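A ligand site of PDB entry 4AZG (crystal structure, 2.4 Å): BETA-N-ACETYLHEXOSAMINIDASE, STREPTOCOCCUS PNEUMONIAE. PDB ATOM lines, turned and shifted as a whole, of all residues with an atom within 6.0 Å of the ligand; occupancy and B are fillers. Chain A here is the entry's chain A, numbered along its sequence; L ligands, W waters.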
ATOM      1  N   ASP A  17      12.753  19.854   4.130  1.00  0.00           N
ATOM      2  CA  ASP A  17      11.542  20.583   4.477  1.00  0.00           C
ATOM      3  C   ASP A  17      11.524  21.910   3.738  1.00  0.00           C
ATOM      4  O   ASP A  17      11.942  22.931   4.269  1.00  0.00           O
ATOM      5  CB  ASP A  17      11.460  20.743   6.005  1.00  0.00           C
ATOM      6  CG  ASP A  17      10.244  21.543   6.484  1.00  0.00           C
ATOM      7  OD1 ASP A  17       9.291  21.801   5.709  1.00  0.00           O
ATOM      8  OD2 ASP A  17      10.266  21.930   7.674  1.00  0.00           O
ATOM      9  N   ARG A  20       8.130  24.652   5.043  1.00  0.00           N
ATOM     10  CA  ARG A  20       8.294  25.769   5.981  1.00  0.00           C
ATOM     11  C   ARG A  20       9.162  26.894   5.403  1.00  0.00           C
ATOM     12  O   ARG A  20       8.960  28.089   5.733  1.00  0.00           O
ATOM     13  CB  ARG A  20       8.861  25.285   7.325  1.00  0.00           C
ATOM     14  CG  ARG A  20       7.876  24.479   8.162  1.00  0.00           C
ATOM     15  CD  ARG A  20       8.474  24.143   9.529  1.00  0.00           C
ATOM     16  NE  ARG A  20       7.557  23.423  10.445  1.00  0.00           N
ATOM     17  CZ  ARG A  20       7.634  22.116  10.723  1.00  0.00           C
ATOM     18  NH1 ARG A  20       8.544  21.343  10.147  1.00  0.00           N
ATOM     19  NH2 ARG A  20       6.788  21.583  11.588  1.00  0.00           N
ATOM     20  N   ASN A  49       4.198  21.909   3.843  1.00  0.00           N
ATOM     21  CA  ASN A  49       4.407  21.575   5.241  1.00  0.00           C
ATOM     22  C   ASN A  49       4.377  22.931   5.960  1.00  0.00           C
ATOM     23  O   ASN A  49       5.371  23.669   5.941  1.00  0.00           O
ATOM     24  CB  ASN A  49       5.768  20.887   5.429  1.00  0.00           C
ATOM     25  CG  ASN A  49       5.894  20.178   6.777  1.00  0.00           C
ATOM     26  OD1 ASN A  49       4.981  19.419   7.188  1.00  0.00           O
ATOM     27  ND2 ASN A  49       7.033  20.382   7.461  1.00  0.00           N
ATOM     28  N   HIS A 121      -0.305  20.558   9.675  1.00  0.00           N
ATOM     29  CA  HIS A 121       0.750  21.327   8.998  1.00  0.00           C
ATOM     30  C   HIS A 121       0.257  21.946   7.724  1.00  0.00           C
ATOM     31  O   HIS A 121       0.864  21.766   6.651  1.00  0.00           O
ATOM     32  CB  HIS A 121       1.970  20.436   8.708  1.00  0.00           C
ATOM     33  CG  HIS A 121       2.601  19.844   9.949  1.00  0.00           C
ATOM     34  ND1 HIS A 121       3.494  20.515  10.721  1.00  0.00           N
ATOM     35  CD2 HIS A 121       2.423  18.598  10.557  1.00  0.00           C
ATOM     36  CE1 HIS A 121       3.861  19.743  11.740  1.00  0.00           C
ATOM     37  NE2 HIS A 121       3.203  18.572  11.644  1.00  0.00           N
ATOM     38  N   ASP A 183       0.823  13.735   9.889  1.00  0.00           N
ATOM     39  CA  ASP A 183       1.455  13.836  11.210  1.00  0.00           C
ATOM     40  C   ASP A 183       0.862  14.973  12.081  1.00  0.00           C
ATOM     41  O   ASP A 183       0.368  15.973  11.562  1.00  0.00           O
ATOM     42  CB  ASP A 183       2.978  14.010  11.080  1.00  0.00           C
ATOM     43  CG  ASP A 183       3.378  15.294  10.365  1.00  0.00           C
ATOM     44  OD1 ASP A 183       2.770  15.585   9.293  1.00  0.00           O
ATOM     45  OD2 ASP A 183       4.298  15.986  10.864  1.00  0.00           O
ATOM     46  N   GLU A 184       0.883  14.774  13.410  1.00  0.00           N
ATOM     47  CA  GLU A 184       0.606  15.825  14.407  1.00  0.00           C
ATOM     48  C   GLU A 184      -0.685  16.600  14.216  1.00  0.00           C
ATOM     49  O   GLU A 184      -0.663  17.842  14.140  1.00  0.00           O
ATOM     50  CB  GLU A 184       1.775  16.804  14.478  1.00  0.00           C
ATOM     51  CG  GLU A 184       3.099  16.106  14.653  1.00  0.00           C
ATOM     52  CD  GLU A 184       4.241  17.061  14.844  1.00  0.00           C
ATOM     53  OE1 GLU A 184       4.561  17.810  13.890  1.00  0.00           O
ATOM     54  OE2 GLU A 184       4.831  17.039  15.945  1.00  0.00           O
ATOM     55  N   ALA A 192      -0.308  19.099  21.695  1.00  0.00           N
ATOM     56  CA  ALA A 192       0.263  17.903  21.081  1.00  0.00           C
ATOM     57  C   ALA A 192      -0.368  16.619  21.613  1.00  0.00           C
ATOM     58  O   ALA A 192       0.318  15.655  21.968  1.00  0.00           O
ATOM     59  CB  ALA A 192       1.785  17.898  21.258  1.00  0.00           C
ATOM     60  N   PHE A 228       3.093   9.632   7.180  1.00  0.00           N
ATOM     61  CA  PHE A 228       3.714   9.449   8.518  1.00  0.00           C
ATOM     62  C   PHE A 228       2.861   8.492   9.373  1.00  0.00           C
ATOM     63  O   PHE A 228       1.641   8.407   9.212  1.00  0.00           O
ATOM     64  CB  PHE A 228       3.944  10.799   9.204  1.00  0.00           C
ATOM     65  CG  PHE A 228       4.872  11.707   8.430  1.00  0.00           C
ATOM     66  CD1 PHE A 228       6.219  11.337   8.199  1.00  0.00           C
ATOM     67  CD2 PHE A 228       4.420  12.907   7.902  1.00  0.00           C
ATOM     68  CE1 PHE A 228       7.075  12.143   7.471  1.00  0.00           C
ATOM     69  CE2 PHE A 228       5.274  13.725   7.162  1.00  0.00           C
ATOM     70  CZ  PHE A 228       6.602  13.336   6.948  1.00  0.00           C
ATOM     71  N   ASP A 230       1.958   8.614  12.601  1.00  0.00           N
ATOM     72  CA  ASP A 230       1.208   9.110  13.784  1.00  0.00           C
ATOM     73  C   ASP A 230      -0.253   8.640  13.893  1.00  0.00           C
ATOM     74  O   ASP A 230      -0.681   8.156  14.950  1.00  0.00           O
ATOM     75  CB  ASP A 230       1.196  10.639  13.890  1.00  0.00           C
ATOM     76  CG  ASP A 230       2.560  11.280  13.705  1.00  0.00           C
ATOM     77  OD1 ASP A 230       3.411  10.743  12.955  1.00  0.00           O
ATOM     78  OD2 ASP A 230       2.774  12.339  14.319  1.00  0.00           O
ATOM     79  N   TRP A 251       8.652   7.432  12.060  1.00  0.00           N
ATOM     80  CA  TRP A 251       9.691   8.305  12.646  1.00  0.00           C
ATOM     81  C   TRP A 251       9.843   8.189  14.158  1.00  0.00           C
ATOM     82  O   TRP A 251      10.921   8.484  14.702  1.00  0.00           O
ATOM     83  CB  TRP A 251       9.488   9.751  12.178  1.00  0.00           C
ATOM     84  CG  TRP A 251       8.248  10.355  12.734  1.00  0.00           C
ATOM     85  CD1 TRP A 251       6.941  10.186  12.291  1.00  0.00           C
ATOM     86  CD2 TRP A 251       8.142  11.256  13.887  1.00  0.00           C
ATOM     87  NE1 TRP A 251       6.073  10.893  13.077  1.00  0.00           N
ATOM     88  CE2 TRP A 251       6.721  11.547  14.048  1.00  0.00           C
ATOM     89  CE3 TRP A 251       9.063  11.816  14.765  1.00  0.00           C
ATOM     90  CZ2 TRP A 251       6.254  12.387  15.054  1.00  0.00           C
ATOM     91  CZ3 TRP A 251       8.582  12.641  15.776  1.00  0.00           C
ATOM     92  CH2 TRP A 251       7.202  12.932  15.921  1.00  0.00           C
ATOM     93  N   SER A 252       8.787   7.721  14.836  1.00  0.00           N
ATOM     94  CA  SER A 252       8.718   7.720  16.297  1.00  0.00           C
ATOM     95  C   SER A 252       7.432   7.068  16.801  1.00  0.00           C
ATOM     96  O   SER A 252       6.379   7.141  16.132  1.00  0.00           O
ATOM     97  CB  SER A 252       8.791   9.148  16.828  1.00  0.00           C
ATOM     98  OG  SER A 252       8.687   9.181  18.237  1.00  0.00           O
ATOM     99  N   GLY A 254       6.210   8.229  19.593  1.00  0.00           N
ATOM    100  CA  GLY A 254       5.621   9.311  20.392  1.00  0.00           C
ATOM    101  C   GLY A 254       6.146   9.376  21.814  1.00  0.00           C
ATOM    102  O   GLY A 254       7.141   8.731  22.146  1.00  0.00           O
ATOM    103  N   TRP A 255       5.452  10.178  22.622  1.00  0.00           N
ATOM    104  CA  TRP A 255       5.934  10.598  23.940  1.00  0.00           C
ATOM    105  C   TRP A 255       4.840  10.431  24.931  1.00  0.00           C
ATOM    106  O   TRP A 255       3.751   9.972  24.569  1.00  0.00           O
ATOM    107  CB  TRP A 255       6.309  12.076  23.850  1.00  0.00           C
ATOM    108  CG  TRP A 255       6.984  12.434  22.555  1.00  0.00           C
ATOM    109  CD1 TRP A 255       6.385  12.744  21.336  1.00  0.00           C
ATOM    110  CD2 TRP A 255       8.441  12.537  22.304  1.00  0.00           C
ATOM    111  NE1 TRP A 255       7.333  13.021  20.377  1.00  0.00           N
ATOM    112  CE2 TRP A 255       8.587  12.907  20.894  1.00  0.00           C
ATOM    113  CE3 TRP A 255       9.580  12.355  23.082  1.00  0.00           C
ATOM    114  CZ2 TRP A 255       9.835  13.087  20.310  1.00  0.00           C
ATOM    115  CZ3 TRP A 255      10.833  12.539  22.476  1.00  0.00           C
ATOM    116  CH2 TRP A 255      10.952  12.897  21.133  1.00  0.00           C
ATOM    117  N   TYR A 258       1.232  10.670  23.828  1.00  0.00           N
ATOM    118  CA  TYR A 258       1.179  10.690  22.369  1.00  0.00           C
ATOM    119  C   TYR A 258       1.460   9.243  21.979  1.00  0.00           C
ATOM    120  O   TYR A 258       2.564   8.904  21.530  1.00  0.00           O
ATOM    121  CB  TYR A 258       2.222  11.679  21.811  1.00  0.00           C
ATOM    122  CG  TYR A 258       1.998  12.083  20.363  1.00  0.00           C
ATOM    123  CD1 TYR A 258       0.848  12.796  19.989  1.00  0.00           C
ATOM    124  CD2 TYR A 258       2.951  11.787  19.365  1.00  0.00           C
ATOM    125  CE1 TYR A 258       0.633  13.155  18.660  1.00  0.00           C
ATOM    126  CE2 TYR A 258       2.751  12.162  18.042  1.00  0.00           C
ATOM    127  CZ  TYR A 258       1.590  12.836  17.696  1.00  0.00           C
ATOM    128  OH  TYR A 258       1.362  13.211  16.376  1.00  0.00           O
ATOM    129  N   TYR A 281      17.094  13.075  12.640  1.00  0.00           N
ATOM    130  CA  TYR A 281      16.591  14.449  12.438  1.00  0.00           C
ATOM    131  C   TYR A 281      17.651  15.550  12.656  1.00  0.00           C
ATOM    132  O   TYR A 281      18.454  15.485  13.593  1.00  0.00           O
ATOM    133  CB  TYR A 281      15.413  14.725  13.346  1.00  0.00           C
ATOM    134  CG  TYR A 281      14.090  14.178  12.877  1.00  0.00           C
ATOM    135  CD1 TYR A 281      14.020  13.214  11.850  1.00  0.00           C
ATOM    136  CD2 TYR A 281      12.899  14.590  13.478  1.00  0.00           C
ATOM    137  CE1 TYR A 281      12.801  12.720  11.419  1.00  0.00           C
ATOM    138  CE2 TYR A 281      11.668  14.083  13.061  1.00  0.00           C
ATOM    139  CZ  TYR A 281      11.626  13.163  12.034  1.00  0.00           C
ATOM    140  OH  TYR A 281      10.424  12.642  11.615  1.00  0.00           O
ATOM    141  N   ILE A 283      17.317  19.863  12.661  1.00  0.00           N
ATOM    142  CA  ILE A 283      16.451  21.035  12.510  1.00  0.00           C
ATOM    143  C   ILE A 283      17.397  22.194  12.305  1.00  0.00           C
ATOM    144  O   ILE A 283      18.292  22.408  13.132  1.00  0.00           O
ATOM    145  CB  ILE A 283      15.601  21.286  13.788  1.00  0.00           C
ATOM    146  CG1 ILE A 283      14.581  20.180  13.974  1.00  0.00           C
ATOM    147  CG2 ILE A 283      14.925  22.659  13.783  1.00  0.00           C
ATOM    148  CD1 ILE A 283      14.783  19.405  15.261  1.00  0.00           C
ATOM    149  N   TRP A 330      14.780  19.346   8.718  1.00  0.00           N
ATOM    150  CA  TRP A 330      13.577  20.125   9.025  1.00  0.00           C
ATOM    151  C   TRP A 330      13.873  21.587   9.245  1.00  0.00           C
ATOM    152  O   TRP A 330      15.006  21.975   9.561  1.00  0.00           O
ATOM    153  CB  TRP A 330      12.895  19.571  10.261  1.00  0.00           C
ATOM    154  CG  TRP A 330      12.499  18.123  10.145  1.00  0.00           C
ATOM    155  CD1 TRP A 330      13.162  17.011  10.650  1.00  0.00           C
ATOM    156  CD2 TRP A 330      11.313  17.583   9.472  1.00  0.00           C
ATOM    157  NE1 TRP A 330      12.504  15.847  10.337  1.00  0.00           N
ATOM    158  CE2 TRP A 330      11.373  16.126   9.623  1.00  0.00           C
ATOM    159  CE3 TRP A 330      10.259  18.142   8.753  1.00  0.00           C
ATOM    160  CZ2 TRP A 330      10.388  15.281   9.118  1.00  0.00           C
ATOM    161  CZ3 TRP A 330       9.280  17.289   8.237  1.00  0.00           C
ATOM    162  CH2 TRP A 330       9.344  15.894   8.419  1.00  0.00           C
ATOM    163  N   ALA A 331      12.856  22.430   9.077  1.00  0.00           N
ATOM    164  CA  ALA A 331      13.041  23.876   9.211  1.00  0.00           C
ATOM    165  C   ALA A 331      12.023  24.505  10.152  1.00  0.00           C
ATOM    166  O   ALA A 331      11.460  25.554   9.859  1.00  0.00           O
ATOM    167  CB  ALA A 331      13.034  24.549   7.843  1.00  0.00           C
ATOM    168  N   ASP A 332      11.800  23.832  11.295  1.00  0.00           N
ATOM    169  CA  ASP A 332      10.915  24.301  12.378  1.00  0.00           C
ATOM    170  C   ASP A 332      10.932  25.820  12.594  1.00  0.00           C
ATOM    171  O   ASP A 332       9.880  26.448  12.742  1.00  0.00           O
ATOM    172  CB  ASP A 332      11.250  23.577  13.690  1.00  0.00           C
ATOM    173  CG  ASP A 332      11.012  22.077  13.582  1.00  0.00           C
ATOM    174  OD1 ASP A 332      11.165  21.527  12.467  1.00  0.00           O
ATOM    175  OD2 ASP A 332      10.659  21.454  14.611  1.00  0.00           O
HETATM  176  C1  LIG L   1       6.944  13.665  11.121  1.00  0.00           C
HETATM  177  C2  LIG L   1       7.710  14.764  11.860  1.00  0.00           C
HETATM  178  O1  LIG L   1       8.940  14.715  11.990  1.00  0.00           O
HETATM  179  N1  LIG L   1       6.935  15.772  12.276  1.00  0.00           N
HETATM  180  C3  LIG L   1       7.409  16.973  12.975  1.00  0.00           C
HETATM  181  C4  LIG L   1       8.097  17.913  11.951  1.00  0.00           C
HETATM  182  O2  LIG L   1       7.154  18.805  11.325  1.00  0.00           O
HETATM  183  C5  LIG L   1       9.272  18.655  12.592  1.00  0.00           C
HETATM  184  O3  LIG L   1       9.858  19.478  11.611  1.00  0.00           O
HETATM  185  C6  LIG L   1      10.298  17.644  13.093  1.00  0.00           C
HETATM  186  C7  LIG L   1      11.490  18.220  13.810  1.00  0.00           C
HETATM  187  O4  LIG L   1      11.074  18.831  15.032  1.00  0.00           O
HETATM  188  O5  LIG L   1       9.763  16.818  14.088  1.00  0.00           O
HETATM  189  C8  LIG L   1       8.397  16.601  14.112  1.00  0.00           C
HETATM  190  N2  LIG L   1       7.919  16.025  15.222  1.00  0.00           N
HETATM  191  O6  LIG L   1       8.884  15.783  16.186  1.00  0.00           O
HETATM  192  C9  LIG L   1       8.351  15.599  17.433  1.00  0.00           C
HETATM  193  O7  LIG L   1       9.011  15.025  18.299  1.00  0.00           O
HETATM  194  N3  LIG L   1       7.113  16.051  17.625  1.00  0.00           N
HETATM  195  C10 LIG L   1       6.377  15.912  18.737  1.00  0.00           C
HETATM  196  C11 LIG L   1       5.229  15.098  18.667  1.00  0.00           C
HETATM  197  C12 LIG L   1       4.408  14.914  19.778  1.00  0.00           C
HETATM  198  C13 LIG L   1       4.736  15.560  20.966  1.00  0.00           C
HETATM  199  C14 LIG L   1       5.879  16.384  21.056  1.00  0.00           C
HETATM  200  C15 LIG L   1       6.707  16.575  19.943  1.00  0.00           C
HETATM  201  O   HOH W   1       5.701  17.679   9.333  1.00  0.00           O
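The indole nitrogen (NE1) of Trp 255 lies close to an oxygen (O7) of the ligand. OH of Tyr 281 is in hydrogen-bond range of O1 of the ligand (2.6 Å). The guanidinium group of Arg 20 is in hydrogen-bond range of an oxygen (O3) of the ligand, at 2.7 Å. The side-chain carboxylate (OE2) of Glu 184 is in hydrogen-bond range of a nitrogen (N3) of the ligand, at 3.0 Å. OD1 of Asp 332 is in hydrogen-bond range of O3 of the ligand. The side-chain carboxylate of Asp 183 is in hydrogen-bond range of a nitrogen (N1) of the ligand.
OH of Tyr 258 is in hydrogen-bond range of OD2 of Asp 230, at 2.6 Å. NE2 of His 121 sits at hydrogen-bond distance from OD2 of Asp 183 (2.9 Å). The backbone carbonyl oxygen (O) of Asn 49 lies within hydrogen-bond range of the backbone NH (N) of Arg 20 (3.1 Å). The side-chain carboxylate (OE1) of Glu 184 is in hydrogen-bond range of a ring nitrogen (NE2) of His 121 (2.7 Å). The indole nitrogen (NE1) of Trp 251 lies within hydrogen-bond range of the side-chain carboxylate (OD1) of Asp 230 (2.7 Å). The side-chain carboxylate of Asp 230 is in hydrogen-bond range of the backbone NH of Glu 184. The guanidinium group (NH1) of Arg 20 is in salt-bridge range of the side-chain carboxylate (OD1) of Asp 332. OH of Tyr 258 lies close to N of Glu 184, 3.4 Å away.
His 121 touches the ligand (CE1 to O2, 3.4 Å). Ala 192 touches the ligand (CB to C13, 3.8 Å). Phe 228 touches the ligand (CD1 to C1, 3.8 Å). Trp 251 touches the ligand. Tyr 258 touches the ligand. Ile 283 touches the ligand (CG1 to C7, 3.7 Å). CE3 of Trp 330 touches O3 of the ligand (3.2 Å). Hydrophobic or aromatic side chains that line the ligand: His 121, Ala 192, Phe 228, Trp 251, Trp 255, Tyr 258, Tyr 281, Ile 283 and Trp 330. Along chain A the residues within 4 Å of the ligand span positions 20 to 332. The nearest printed residue that does not touch the ligand is Asn 49 (4.2 Å).
Water W1 lies within hydrogen-bond range of OD2 of Asp 183 (2.7 Å), O2 of the ligand (2.7 Å) and OD1 of Asn 49 (2.9 Å).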
